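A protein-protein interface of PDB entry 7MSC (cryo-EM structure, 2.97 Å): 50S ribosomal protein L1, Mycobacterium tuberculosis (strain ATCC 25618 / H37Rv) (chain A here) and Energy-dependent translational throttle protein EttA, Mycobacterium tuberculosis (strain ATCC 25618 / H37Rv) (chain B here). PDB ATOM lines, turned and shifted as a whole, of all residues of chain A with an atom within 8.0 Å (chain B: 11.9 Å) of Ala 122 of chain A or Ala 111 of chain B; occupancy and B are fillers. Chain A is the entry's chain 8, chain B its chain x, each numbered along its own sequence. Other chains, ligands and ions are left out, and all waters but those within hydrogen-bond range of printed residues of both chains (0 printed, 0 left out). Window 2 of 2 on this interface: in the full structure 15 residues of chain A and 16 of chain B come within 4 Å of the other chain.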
ATOM      1  N   ASP A  98       2.906  13.563 -15.768  1.00  0.00           N
ATOM      2  CA  ASP A  98       3.114  14.895 -15.208  1.00  0.00           C
ATOM      3  C   ASP A  98       2.605  15.023 -13.775  1.00  0.00           C
ATOM      4  O   ASP A  98       3.029  15.940 -13.064  1.00  0.00           O
ATOM      5  CB  ASP A  98       2.436  15.935 -16.097  1.00  0.00           C
ATOM      6  CG  ASP A  98       3.104  16.064 -17.446  1.00  0.00           C
ATOM      7  OD1 ASP A  98       4.330  15.849 -17.523  1.00  0.00           O
ATOM      8  OD2 ASP A  98       2.405  16.382 -18.431  1.00  0.00           O
ATOM      9  N   ILE A 101       5.205  14.765 -10.640  1.00  0.00           N
ATOM     10  CA  ILE A 101       5.793  15.952 -10.022  1.00  0.00           C
ATOM     11  C   ILE A 101       5.392  16.046  -8.554  1.00  0.00           C
ATOM     12  O   ILE A 101       6.229  16.290  -7.675  1.00  0.00           O
ATOM     13  CB  ILE A 101       5.369  17.210 -10.807  1.00  0.00           C
ATOM     14  CG1 ILE A 101       5.984  17.211 -12.206  1.00  0.00           C
ATOM     15  CG2 ILE A 101       5.704  18.485 -10.052  1.00  0.00           C
ATOM     16  CD1 ILE A 101       5.419  18.286 -13.110  1.00  0.00           C
ATOM     17  N   ALA A 116      12.605   8.981 -19.434  1.00  0.00           N
ATOM     18  CA  ALA A 116      11.734  10.053 -19.890  1.00  0.00           C
ATOM     19  C   ALA A 116      12.056  10.413 -21.331  1.00  0.00           C
ATOM     20  O   ALA A 116      13.181  10.225 -21.801  1.00  0.00           O
ATOM     21  CB  ALA A 116      11.869  11.293 -19.001  1.00  0.00           C
ATOM     22  N   THR A 117      11.049  10.926 -22.030  1.00  0.00           N
ATOM     23  CA  THR A 117      11.267  11.562 -23.314  1.00  0.00           C
ATOM     24  C   THR A 117      11.856  12.950 -23.080  1.00  0.00           C
ATOM     25  O   THR A 117      11.749  13.493 -21.978  1.00  0.00           O
ATOM     26  CB  THR A 117       9.951  11.665 -24.086  1.00  0.00           C
ATOM     27  OG1 THR A 117       9.080  12.593 -23.432  1.00  0.00           O
ATOM     28  CG2 THR A 117       9.273  10.308 -24.163  1.00  0.00           C
ATOM     29  N   PRO A 118      12.508  13.541 -24.089  1.00  0.00           N
ATOM     30  CA  PRO A 118      12.957  14.936 -23.941  1.00  0.00           C
ATOM     31  C   PRO A 118      11.829  15.942 -23.790  1.00  0.00           C
ATOM     32  O   PRO A 118      12.069  17.048 -23.288  1.00  0.00           O
ATOM     33  CB  PRO A 118      13.754  15.182 -25.227  1.00  0.00           C
ATOM     34  CG  PRO A 118      14.228  13.840 -25.626  1.00  0.00           C
ATOM     35  CD  PRO A 118      13.135  12.895 -25.259  1.00  0.00           C
ATOM     36  N   ASP A 119      10.607  15.603 -24.205  1.00  0.00           N
ATOM     37  CA  ASP A 119       9.476  16.483 -23.945  1.00  0.00           C
ATOM     38  C   ASP A 119       9.066  16.449 -22.479  1.00  0.00           C
ATOM     39  O   ASP A 119       8.630  17.470 -21.936  1.00  0.00           O
ATOM     40  CB  ASP A 119       8.299  16.095 -24.837  1.00  0.00           C
ATOM     41  CG  ASP A 119       8.567  16.367 -26.300  1.00  0.00           C
ATOM     42  OD1 ASP A 119       9.349  17.293 -26.596  1.00  0.00           O
ATOM     43  OD2 ASP A 119       7.997  15.656 -27.152  1.00  0.00           O
ATOM     44  N   GLN A 120       9.203  15.295 -21.821  1.00  0.00           N
ATOM     45  CA  GLN A 120       8.843  15.186 -20.413  1.00  0.00           C
ATOM     46  C   GLN A 120       9.881  15.800 -19.486  1.00  0.00           C
ATOM     47  O   GLN A 120       9.542  16.162 -18.357  1.00  0.00           O
ATOM     48  CB  GLN A 120       8.624  13.721 -20.030  1.00  0.00           C
ATOM     49  CG  GLN A 120       7.410  13.093 -20.678  1.00  0.00           C
ATOM     50  CD  GLN A 120       6.117  13.694 -20.181  1.00  0.00           C
ATOM     51  OE1 GLN A 120       5.955  13.944 -18.989  1.00  0.00           O
ATOM     52  NE2 GLN A 120       5.193  13.949 -21.097  1.00  0.00           N
ATOM     53  N   MET A 121      11.128  15.954 -19.945  1.00  0.00           N
ATOM     54  CA  MET A 121      12.204  16.466 -19.100  1.00  0.00           C
ATOM     55  C   MET A 121      12.080  17.950 -18.790  1.00  0.00           C
ATOM     56  O   MET A 121      12.870  18.461 -17.990  1.00  0.00           O
ATOM     57  CB  MET A 121      13.561  16.201 -19.753  1.00  0.00           C
ATOM     58  CG  MET A 121      13.970  14.740 -19.772  1.00  0.00           C
ATOM     59  SD  MET A 121      14.119  14.075 -18.103  1.00  0.00           S
ATOM     60  CE  MET A 121      15.540  14.981 -17.497  1.00  0.00           C
ATOM     61  N   ALA A 122      11.121  18.647 -19.401  1.00  0.00           N
ATOM     62  CA  ALA A 122      10.929  20.063 -19.125  1.00  0.00           C
ATOM     63  C   ALA A 122      10.404  20.303 -17.715  1.00  0.00           C
ATOM     64  O   ALA A 122      10.642  21.371 -17.139  1.00  0.00           O
ATOM     65  CB  ALA A 122       9.973  20.667 -20.155  1.00  0.00           C
ATOM     66  N   LYS A 123       9.704  19.327 -17.141  1.00  0.00           N
ATOM     67  CA  LYS A 123       9.082  19.491 -15.838  1.00  0.00           C
ATOM     68  C   LYS A 123       9.625  18.536 -14.783  1.00  0.00           C
ATOM     69  O   LYS A 123       9.189  18.596 -13.628  1.00  0.00           O
ATOM     70  CB  LYS A 123       7.562  19.324 -15.970  1.00  0.00           C
ATOM     71  CG  LYS A 123       6.919  20.400 -16.824  1.00  0.00           C
ATOM     72  CD  LYS A 123       5.409  20.326 -16.801  1.00  0.00           C
ATOM     73  CE  LYS A 123       4.897  19.179 -17.650  1.00  0.00           C
ATOM     74  NZ  LYS A 123       3.413  19.220 -17.735  1.00  0.00           N
ATOM     75  N   VAL A 124      10.561  17.661 -15.143  1.00  0.00           N
ATOM     76  CA  VAL A 124      11.201  16.768 -14.182  1.00  0.00           C
ATOM     77  C   VAL A 124      12.438  17.417 -13.571  1.00  0.00           C
ATOM     78  O   VAL A 124      12.697  17.270 -12.373  1.00  0.00           O
ATOM     79  CB  VAL A 124      11.539  15.433 -14.878  1.00  0.00           C
ATOM     80  CG1 VAL A 124      12.253  14.472 -13.940  1.00  0.00           C
ATOM     81  CG2 VAL A 124      10.280  14.797 -15.423  1.00  0.00           C
ATOM     82  N   GLY A 125      13.185  18.172 -14.380  1.00  0.00           N
ATOM     83  CA  GLY A 125      14.422  18.794 -13.939  1.00  0.00           C
ATOM     84  C   GLY A 125      14.250  19.875 -12.892  1.00  0.00           C
ATOM     85  O   GLY A 125      15.200  20.163 -12.157  1.00  0.00           O
ATOM     86  N   ARG A 126      13.067  20.489 -12.812  1.00  0.00           N
ATOM     87  CA  ARG A 126      12.800  21.391 -11.696  1.00  0.00           C
ATOM     88  C   ARG A 126      12.590  20.611 -10.408  1.00  0.00           C
ATOM     89  O   ARG A 126      12.886  21.116  -9.320  1.00  0.00           O
ATOM     90  CB  ARG A 126      11.584  22.274 -11.985  1.00  0.00           C
ATOM     91  CG  ARG A 126      11.866  23.464 -12.894  1.00  0.00           C
ATOM     92  CD  ARG A 126      11.695  23.121 -14.368  1.00  0.00           C
ATOM     93  NE  ARG A 126      10.330  22.704 -14.670  1.00  0.00           N
ATOM     94  CZ  ARG A 126       9.342  23.545 -14.955  1.00  0.00           C
ATOM     95  NH1 ARG A 126       8.129  23.085 -15.211  1.00  0.00           N
ATOM     96  NH2 ARG A 126       9.567  24.853 -14.983  1.00  0.00           N
ATOM     97  N   ILE A 127      12.086  19.380 -10.514  1.00  0.00           N
ATOM     98  CA  ILE A 127      11.912  18.521  -9.346  1.00  0.00           C
ATOM     99  C   ILE A 127      13.202  17.792  -9.005  1.00  0.00           C
ATOM    100  O   ILE A 127      13.353  17.286  -7.884  1.00  0.00           O
ATOM    101  CB  ILE A 127      10.698  17.620  -9.651  1.00  0.00           C
ATOM    102  CG1 ILE A 127       9.510  18.500 -10.039  1.00  0.00           C
ATOM    103  CG2 ILE A 127      10.264  16.781  -8.451  1.00  0.00           C
ATOM    104  CD1 ILE A 127       9.096  19.480  -8.942  1.00  0.00           C
ATOM    105  N   ARG B 102      22.060  28.177 -16.754  1.00  0.00           N
ATOM    106  CA  ARG B 102      21.871  27.594 -18.073  1.00  0.00           C
ATOM    107  C   ARG B 102      21.008  26.346 -18.033  1.00  0.00           C
ATOM    108  O   ARG B 102      20.247  26.102 -18.971  1.00  0.00           O
ATOM    109  CB  ARG B 102      23.233  27.261 -18.701  1.00  0.00           C
ATOM    110  CG  ARG B 102      23.205  26.730 -20.126  1.00  0.00           C
ATOM    111  CD  ARG B 102      22.725  27.778 -21.108  1.00  0.00           C
ATOM    112  NE  ARG B 102      22.762  27.290 -22.482  1.00  0.00           N
ATOM    113  CZ  ARG B 102      21.782  26.604 -23.060  1.00  0.00           C
ATOM    114  NH1 ARG B 102      20.676  26.319 -22.387  1.00  0.00           N
ATOM    115  NH2 ARG B 102      21.909  26.201 -24.316  1.00  0.00           N
ATOM    116  N   PHE B 103      21.079  25.576 -16.944  1.00  0.00           N
ATOM    117  CA  PHE B 103      20.269  24.370 -16.829  1.00  0.00           C
ATOM    118  C   PHE B 103      18.798  24.692 -16.593  1.00  0.00           C
ATOM    119  O   PHE B 103      17.927  23.926 -17.017  1.00  0.00           O
ATOM    120  CB  PHE B 103      20.805  23.484 -15.707  1.00  0.00           C
ATOM    121  CG  PHE B 103      20.085  22.179 -15.574  1.00  0.00           C
ATOM    122  CD1 PHE B 103      20.337  21.150 -16.460  1.00  0.00           C
ATOM    123  CD2 PHE B 103      19.153  21.980 -14.567  1.00  0.00           C
ATOM    124  CE1 PHE B 103      19.676  19.945 -16.347  1.00  0.00           C
ATOM    125  CE2 PHE B 103      18.489  20.779 -14.449  1.00  0.00           C
ATOM    126  CZ  PHE B 103      18.750  19.759 -15.340  1.00  0.00           C
ATOM    127  N   ASN B 104      18.491  25.796 -15.912  1.00  0.00           N
ATOM    128  CA  ASN B 104      17.094  26.199 -15.825  1.00  0.00           C
ATOM    129  C   ASN B 104      16.615  26.895 -17.091  1.00  0.00           C
ATOM    130  O   ASN B 104      15.405  26.947 -17.336  1.00  0.00           O
ATOM    131  CB  ASN B 104      16.863  27.084 -14.593  1.00  0.00           C
ATOM    132  CG  ASN B 104      17.753  28.319 -14.566  1.00  0.00           C
ATOM    133  OD1 ASN B 104      18.523  28.579 -15.486  1.00  0.00           O
ATOM    134  ND2 ASN B 104      17.644  29.089 -13.490  1.00  0.00           N
ATOM    135  N   GLU B 105      17.541  27.435 -17.888  1.00  0.00           N
ATOM    136  CA  GLU B 105      17.185  27.996 -19.186  1.00  0.00           C
ATOM    137  C   GLU B 105      16.744  26.908 -20.153  1.00  0.00           C
ATOM    138  O   GLU B 105      15.756  27.072 -20.877  1.00  0.00           O
ATOM    139  CB  GLU B 105      18.370  28.762 -19.766  1.00  0.00           C
ATOM    140  CG  GLU B 105      18.102  29.403 -21.113  1.00  0.00           C
ATOM    141  CD  GLU B 105      19.316  30.125 -21.662  1.00  0.00           C
ATOM    142  OE1 GLU B 105      20.373  30.098 -21.000  1.00  0.00           O
ATOM    143  OE2 GLU B 105      19.216  30.715 -22.758  1.00  0.00           O
ATOM    144  N   VAL B 106      17.461  25.782 -20.168  1.00  0.00           N
ATOM    145  CA  VAL B 106      17.148  24.690 -21.086  1.00  0.00           C
ATOM    146  C   VAL B 106      15.979  23.850 -20.591  1.00  0.00           C
ATOM    147  O   VAL B 106      15.476  22.997 -21.330  1.00  0.00           O
ATOM    148  CB  VAL B 106      18.438  23.869 -21.294  1.00  0.00           C
ATOM    149  CG1 VAL B 106      18.714  22.981 -20.095  1.00  0.00           C
ATOM    150  CG2 VAL B 106      18.433  23.099 -22.613  1.00  0.00           C
ATOM    151  N   ALA B 107      15.503  24.092 -19.368  1.00  0.00           N
ATOM    152  CA  ALA B 107      14.326  23.400 -18.858  1.00  0.00           C
ATOM    153  C   ALA B 107      13.036  23.839 -19.537  1.00  0.00           C
ATOM    154  O   ALA B 107      12.021  23.153 -19.391  1.00  0.00           O
ATOM    155  CB  ALA B 107      14.203  23.609 -17.349  1.00  0.00           C
ATOM    156  N   GLU B 108      13.036  24.965 -20.246  1.00  0.00           N
ATOM    157  CA  GLU B 108      11.904  25.366 -21.070  1.00  0.00           C
ATOM    158  C   GLU B 108      12.275  25.675 -22.508  1.00  0.00           C
ATOM    159  O   GLU B 108      11.378  25.710 -23.359  1.00  0.00           O
ATOM    160  CB  GLU B 108      11.197  26.594 -20.472  1.00  0.00           C
ATOM    161  CG  GLU B 108      10.433  26.328 -19.182  1.00  0.00           C
ATOM    162  CD  GLU B 108      11.306  26.419 -17.948  1.00  0.00           C
ATOM    163  OE1 GLU B 108      12.501  26.760 -18.082  1.00  0.00           O
ATOM    164  OE2 GLU B 108      10.796  26.151 -16.841  1.00  0.00           O
ATOM    165  N   LEU B 109      13.554  25.900 -22.812  1.00  0.00           N
ATOM    166  CA  LEU B 109      13.967  26.176 -24.181  1.00  0.00           C
ATOM    167  C   LEU B 109      14.062  24.902 -25.006  1.00  0.00           C
ATOM    168  O   LEU B 109      13.756  24.922 -26.202  1.00  0.00           O
ATOM    169  CB  LEU B 109      15.303  26.927 -24.170  1.00  0.00           C
ATOM    170  CG  LEU B 109      15.887  27.556 -25.438  1.00  0.00           C
ATOM    171  CD1 LEU B 109      16.610  28.837 -25.065  1.00  0.00           C
ATOM    172  CD2 LEU B 109      16.860  26.623 -26.140  1.00  0.00           C
ATOM    173  N   MET B 110      14.479  23.793 -24.391  1.00  0.00           N
ATOM    174  CA  MET B 110      14.597  22.528 -25.106  1.00  0.00           C
ATOM    175  C   MET B 110      13.232  21.912 -25.407  1.00  0.00           C
ATOM    176  O   MET B 110      13.112  21.133 -26.360  1.00  0.00           O
ATOM    177  CB  MET B 110      15.489  21.580 -24.289  1.00  0.00           C
ATOM    178  CG  MET B 110      15.826  20.220 -24.894  1.00  0.00           C
ATOM    179  SD  MET B 110      14.692  18.910 -24.402  1.00  0.00           S
ATOM    180  CE  MET B 110      15.223  18.630 -22.716  1.00  0.00           C
ATOM    181  N   ALA B 111      12.196  22.274 -24.644  1.00  0.00           N
ATOM    182  CA  ALA B 111      10.865  21.728 -24.894  1.00  0.00           C
ATOM    183  C   ALA B 111      10.261  22.294 -26.174  1.00  0.00           C
ATOM    184  O   ALA B 111       9.678  21.552 -26.972  1.00  0.00           O
ATOM    185  CB  ALA B 111       9.953  22.008 -23.701  1.00  0.00           C
ATOM    186  N   THR B 112      10.399  23.598 -26.394  1.00  0.00           N
ATOM    187  CA  THR B 112       9.855  24.243 -27.579  1.00  0.00           C
ATOM    188  C   THR B 112      10.808  24.217 -28.770  1.00  0.00           C
ATOM    189  O   THR B 112      10.486  24.803 -29.809  1.00  0.00           O
ATOM    190  CB  THR B 112       9.477  25.694 -27.260  1.00  0.00           C
ATOM    191  OG1 THR B 112       8.824  26.280 -28.392  1.00  0.00           O
ATOM    192  CG2 THR B 112      10.716  26.505 -26.919  1.00  0.00           C
ATOM    193  N   ASP B 113      11.960  23.554 -28.653  1.00  0.00           N
ATOM    194  CA  ASP B 113      12.930  23.515 -29.743  1.00  0.00           C
ATOM    195  C   ASP B 113      13.370  22.091 -30.056  1.00  0.00           C
ATOM    196  O   ASP B 113      12.803  21.127 -29.532  1.00  0.00           O
ATOM    197  CB  ASP B 113      14.157  24.370 -29.413  1.00  0.00           C
ATOM    198  CG  ASP B 113      13.856  25.854 -29.426  1.00  0.00           C
ATOM    199  OD1 ASP B 113      12.969  26.278 -30.196  1.00  0.00           O
ATOM    200  OD2 ASP B 113      14.510  26.598 -28.666  1.00  0.00           O
ATOM    201  N   TYR B 114      14.390  21.954 -30.903  1.00  0.00           N
ATOM    202  CA  TYR B 114      14.815  20.650 -31.392  1.00  0.00           C
ATOM    203  C   TYR B 114      15.621  19.909 -30.331  1.00  0.00           C
ATOM    204  O   TYR B 114      16.562  20.456 -29.749  1.00  0.00           O
ATOM    205  CB  TYR B 114      15.609  20.803 -32.696  1.00  0.00           C
ATOM    206  CG  TYR B 114      16.861  21.656 -32.629  1.00  0.00           C
ATOM    207  CD1 TYR B 114      16.803  23.033 -32.815  1.00  0.00           C
ATOM    208  CD2 TYR B 114      18.108  21.078 -32.436  1.00  0.00           C
ATOM    209  CE1 TYR B 114      17.949  23.810 -32.772  1.00  0.00           C
ATOM    210  CE2 TYR B 114      19.256  21.840 -32.392  1.00  0.00           C
ATOM    211  CZ  TYR B 114      19.173  23.205 -32.562  1.00  0.00           C
ATOM    212  OH  TYR B 114      20.318  23.967 -32.519  1.00  0.00           O
ATOM    213  N   THR B 115      15.211  18.678 -30.051  1.00  0.00           N
ATOM    214  CA  THR B 115      15.763  17.882 -28.954  1.00  0.00           C
ATOM    215  C   THR B 115      16.826  16.890 -29.421  1.00  0.00           C
ATOM    216  O   THR B 115      16.730  15.703 -29.111  1.00  0.00           O
ATOM    217  CB  THR B 115      14.634  17.153 -28.241  1.00  0.00           C
ATOM    218  OG1 THR B 115      14.052  16.198 -29.133  1.00  0.00           O
ATOM    219  CG2 THR B 115      13.558  18.136 -27.820  1.00  0.00           C
ATOM    220  N   ASP B 116      17.848  17.326 -30.161  1.00  0.00           N
ATOM    221  CA  ASP B 116      18.962  16.404 -30.383  1.00  0.00           C
ATOM    222  C   ASP B 116      20.320  17.018 -30.077  1.00  0.00           C
ATOM    223  O   ASP B 116      21.188  16.331 -29.532  1.00  0.00           O
ATOM    224  CB  ASP B 116      18.939  15.830 -31.826  1.00  0.00           C
ATOM    225  CG  ASP B 116      19.019  16.898 -32.904  1.00  0.00           C
ATOM    226  OD1 ASP B 116      18.999  18.100 -32.584  1.00  0.00           O
ATOM    227  OD2 ASP B 116      19.108  16.523 -34.091  1.00  0.00           O
ATOM    228  N   GLU B 117      20.528  18.294 -30.406  1.00  0.00           N
ATOM    229  CA  GLU B 117      21.755  18.967 -29.999  1.00  0.00           C
ATOM    230  C   GLU B 117      21.646  19.489 -28.574  1.00  0.00           C
ATOM    231  O   GLU B 117      22.635  19.474 -27.833  1.00  0.00           O
ATOM    232  CB  GLU B 117      22.082  20.102 -30.971  1.00  0.00           C
ATOM    233  CG  GLU B 117      23.488  20.687 -30.840  1.00  0.00           C
ATOM    234  CD  GLU B 117      23.576  21.826 -29.840  1.00  0.00           C
ATOM    235  OE1 GLU B 117      22.571  22.547 -29.667  1.00  0.00           O
ATOM    236  OE2 GLU B 117      24.647  21.990 -29.217  1.00  0.00           O
ATOM    237  N   LEU B 118      20.458  19.935 -28.172  1.00  0.00           N
ATOM    238  CA  LEU B 118      20.212  20.383 -26.809  1.00  0.00           C
ATOM    239  C   LEU B 118      20.022  19.230 -25.836  1.00  0.00           C
ATOM    240  O   LEU B 118      19.879  19.477 -24.635  1.00  0.00           O
ATOM    241  CB  LEU B 118      18.983  21.292 -26.774  1.00  0.00           C
ATOM    242  CG  LEU B 118      19.117  22.591 -27.563  1.00  0.00           C
ATOM    243  CD1 LEU B 118      17.788  23.312 -27.617  1.00  0.00           C
ATOM    244  CD2 LEU B 118      20.180  23.480 -26.949  1.00  0.00           C
ATOM    245  N   MET B 119      19.996  17.986 -26.325  1.00  0.00           N
ATOM    246  CA  MET B 119      19.920  16.833 -25.438  1.00  0.00           C
ATOM    247  C   MET B 119      21.204  16.670 -24.640  1.00  0.00           C
ATOM    248  O   MET B 119      21.164  16.433 -23.427  1.00  0.00           O
ATOM    249  CB  MET B 119      19.638  15.566 -26.242  1.00  0.00           C
ATOM    250  CG  MET B 119      19.460  14.322 -25.392  1.00  0.00           C
ATOM    251  SD  MET B 119      19.230  12.826 -26.373  1.00  0.00           S
ATOM    252  CE  MET B 119      17.583  13.083 -27.022  1.00  0.00           C
ATOM    253  N   GLU B 120      22.352  16.783 -25.304  1.00  0.00           N
ATOM    254  CA  GLU B 120      23.628  16.716 -24.607  1.00  0.00           C
ATOM    255  C   GLU B 120      24.001  18.039 -23.951  1.00  0.00           C
ATOM    256  O   GLU B 120      24.853  18.053 -23.055  1.00  0.00           O
ATOM    257  CB  GLU B 120      24.724  16.256 -25.576  1.00  0.00           C
ATOM    258  CG  GLU B 120      24.858  17.093 -26.841  1.00  0.00           C
ATOM    259  CD  GLU B 120      25.819  18.257 -26.689  1.00  0.00           C
ATOM    260  OE1 GLU B 120      26.646  18.224 -25.753  1.00  0.00           O
ATOM    261  OE2 GLU B 120      25.747  19.199 -27.504  1.00  0.00           O
ATOM    262  N   GLU B 121      23.389  19.145 -24.376  1.00  0.00           N
ATOM    263  CA  GLU B 121      23.659  20.423 -23.728  1.00  0.00           C
ATOM    264  C   GLU B 121      23.012  20.501 -22.355  1.00  0.00           C
ATOM    265  O   GLU B 121      23.489  21.241 -21.493  1.00  0.00           O
ATOM    266  CB  GLU B 121      23.192  21.578 -24.610  1.00  0.00           C
ATOM    267  CG  GLU B 121      24.027  21.759 -25.868  1.00  0.00           C
ATOM    268  CD  GLU B 121      25.442  22.217 -25.568  1.00  0.00           C
ATOM    269  OE1 GLU B 121      25.632  22.972 -24.590  1.00  0.00           O
ATOM    270  OE2 GLU B 121      26.364  21.819 -26.311  1.00  0.00           O
ATOM    271  N   MET B 122      21.927  19.765 -22.132  1.00  0.00           N
ATOM    272  CA  MET B 122      21.443  19.539 -20.781  1.00  0.00           C
ATOM    273  C   MET B 122      22.032  18.275 -20.181  1.00  0.00           C
ATOM    274  O   MET B 122      21.626  17.869 -19.088  1.00  0.00           O
ATOM    275  CB  MET B 122      19.910  19.500 -20.751  1.00  0.00           C
ATOM    276  CG  MET B 122      19.239  18.402 -21.567  1.00  0.00           C
ATOM    277  SD  MET B 122      18.975  16.834 -20.712  1.00  0.00           S
ATOM    278  CE  MET B 122      17.710  17.315 -19.539  1.00  0.00           C
ATOM    279  N   GLN B 126      24.564  18.530 -16.574  1.00  0.00           N
ATOM    280  CA  GLN B 126      24.152  17.610 -15.526  1.00  0.00           C
ATOM    281  C   GLN B 126      25.307  16.734 -15.056  1.00  0.00           C
ATOM    282  O   GLN B 126      25.266  16.218 -13.935  1.00  0.00           O
ATOM    283  CB  GLN B 126      22.982  16.777 -16.045  1.00  0.00           C
ATOM    284  CG  GLN B 126      22.198  16.009 -15.008  1.00  0.00           C
ATOM    285  CD  GLN B 126      20.986  15.335 -15.618  1.00  0.00           C
ATOM    286  OE1 GLN B 126      20.788  15.376 -16.830  1.00  0.00           O
ATOM    287  NE2 GLN B 126      20.157  14.726 -14.781  1.00  0.00           N
ATOM    288  N   TRP B 135      23.262  20.991  -6.583  1.00  0.00           N
ATOM    289  CA  TRP B 135      21.807  20.897  -6.588  1.00  0.00           C
ATOM    290  C   TRP B 135      21.181  21.644  -5.423  1.00  0.00           C
ATOM    291  O   TRP B 135      20.009  22.026  -5.503  1.00  0.00           O
ATOM    292  CB  TRP B 135      21.360  19.436  -6.552  1.00  0.00           C
ATOM    293  CG  TRP B 135      21.709  18.673  -7.783  1.00  0.00           C
ATOM    294  CD1 TRP B 135      22.740  17.801  -7.943  1.00  0.00           C
ATOM    295  CD2 TRP B 135      21.034  18.731  -9.040  1.00  0.00           C
ATOM    296  NE1 TRP B 135      22.748  17.303  -9.221  1.00  0.00           N
ATOM    297  CE2 TRP B 135      21.708  17.861  -9.916  1.00  0.00           C
ATOM    298  CE3 TRP B 135      19.919  19.428  -9.509  1.00  0.00           C
ATOM    299  CZ2 TRP B 135      21.303  17.670 -11.235  1.00  0.00           C
ATOM    300  CZ3 TRP B 135      19.523  19.243 -10.820  1.00  0.00           C
ATOM    301  CH2 TRP B 135      20.211  18.370 -11.667  1.00  0.00           C
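Of chain A, only Ala 122 comes within 4 Å of Ala 111 of chain B. No residue of chain B comes within 4 Å of Asp 119 of chain A. No residue of chain B comes within 4 Å of Gln 120 of chain A. Of chain B, only Met 122 comes within 4 Å of Met 121 of chain A. No residue of chain B comes within 4 Å of Lys 123 of chain A. No residue of chain B comes within 4 Å of Gly 125 of chain A. Of the printed residues of chain A, Met 110 of chain B touches Pro 118 (3.4 Å). Of the printed residues of chain A, Met 122 of chain B touches Met 121. Asp 98 of chain A touches none of the printed residues of chain B.
The guanidinium group (NH2) of Arg 126 of chain A is in salt-bridge range of the side-chain carboxylate (OE2) of Glu 108 of chain B, at 2.6 Å. The backbone carbonyl oxygen (O) of Pro 118 of chain A lies close to the side-chain sulfur (SD) of Met 110 of chain B (3.4 Å). The backbone carbonyl oxygen (O) of Ala 107 of chain B lies close to the backbone carbonyl oxygen (O) of Ala 122 of chain A, at 3.2 Å.
The backbone carbonyl oxygen of Met 122 of chain B lies close to the side-chain amide oxygen of Gln 126 of chain B, at 3.5 Å. The backbone carbonyl oxygen (O) of Ala 122 of chain A sits at hydrogen-bond distance from the guanidinium group (NE) of Arg 126 of chain A (2.8 Å).
Among the printed residues, merely in contact across the chains: Pro 118 of chain A with Thr 115 of chain B (3.7 Å), Pro 118 of chain A with Met 119 of chain B (3.7 Å), Met 121 of chain A with Met 122 of chain B (3.8 Å), Ala 122 of chain A with Ala 111 of chain B (3.8 Å) and Arg 126 of chain A with Ala 107 of chain B (3.9 Å).
Hydrophobic or aromatic side chains of chain B that line the printed part of chain A: Ala 107, Met 110, Ala 111, Met 119 and Met 122. Of the 14 printed residues of chain A, 4 touch a printed residue of chain B. Hydrophobic or aromatic side chains of chain A that line the printed part of chain B: Pro 118, Met 121 and Ala 122. Along chain A the printed residues that touch a printed residue of chain B span positions 118 to 126. Among the printed residues, Asp or Glu carboxylates within 4 Å of a Lys or Arg side-chain nitrogen of the other chain: Arg 126 of chain A with Glu 108 of chain B (2.6 Å).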
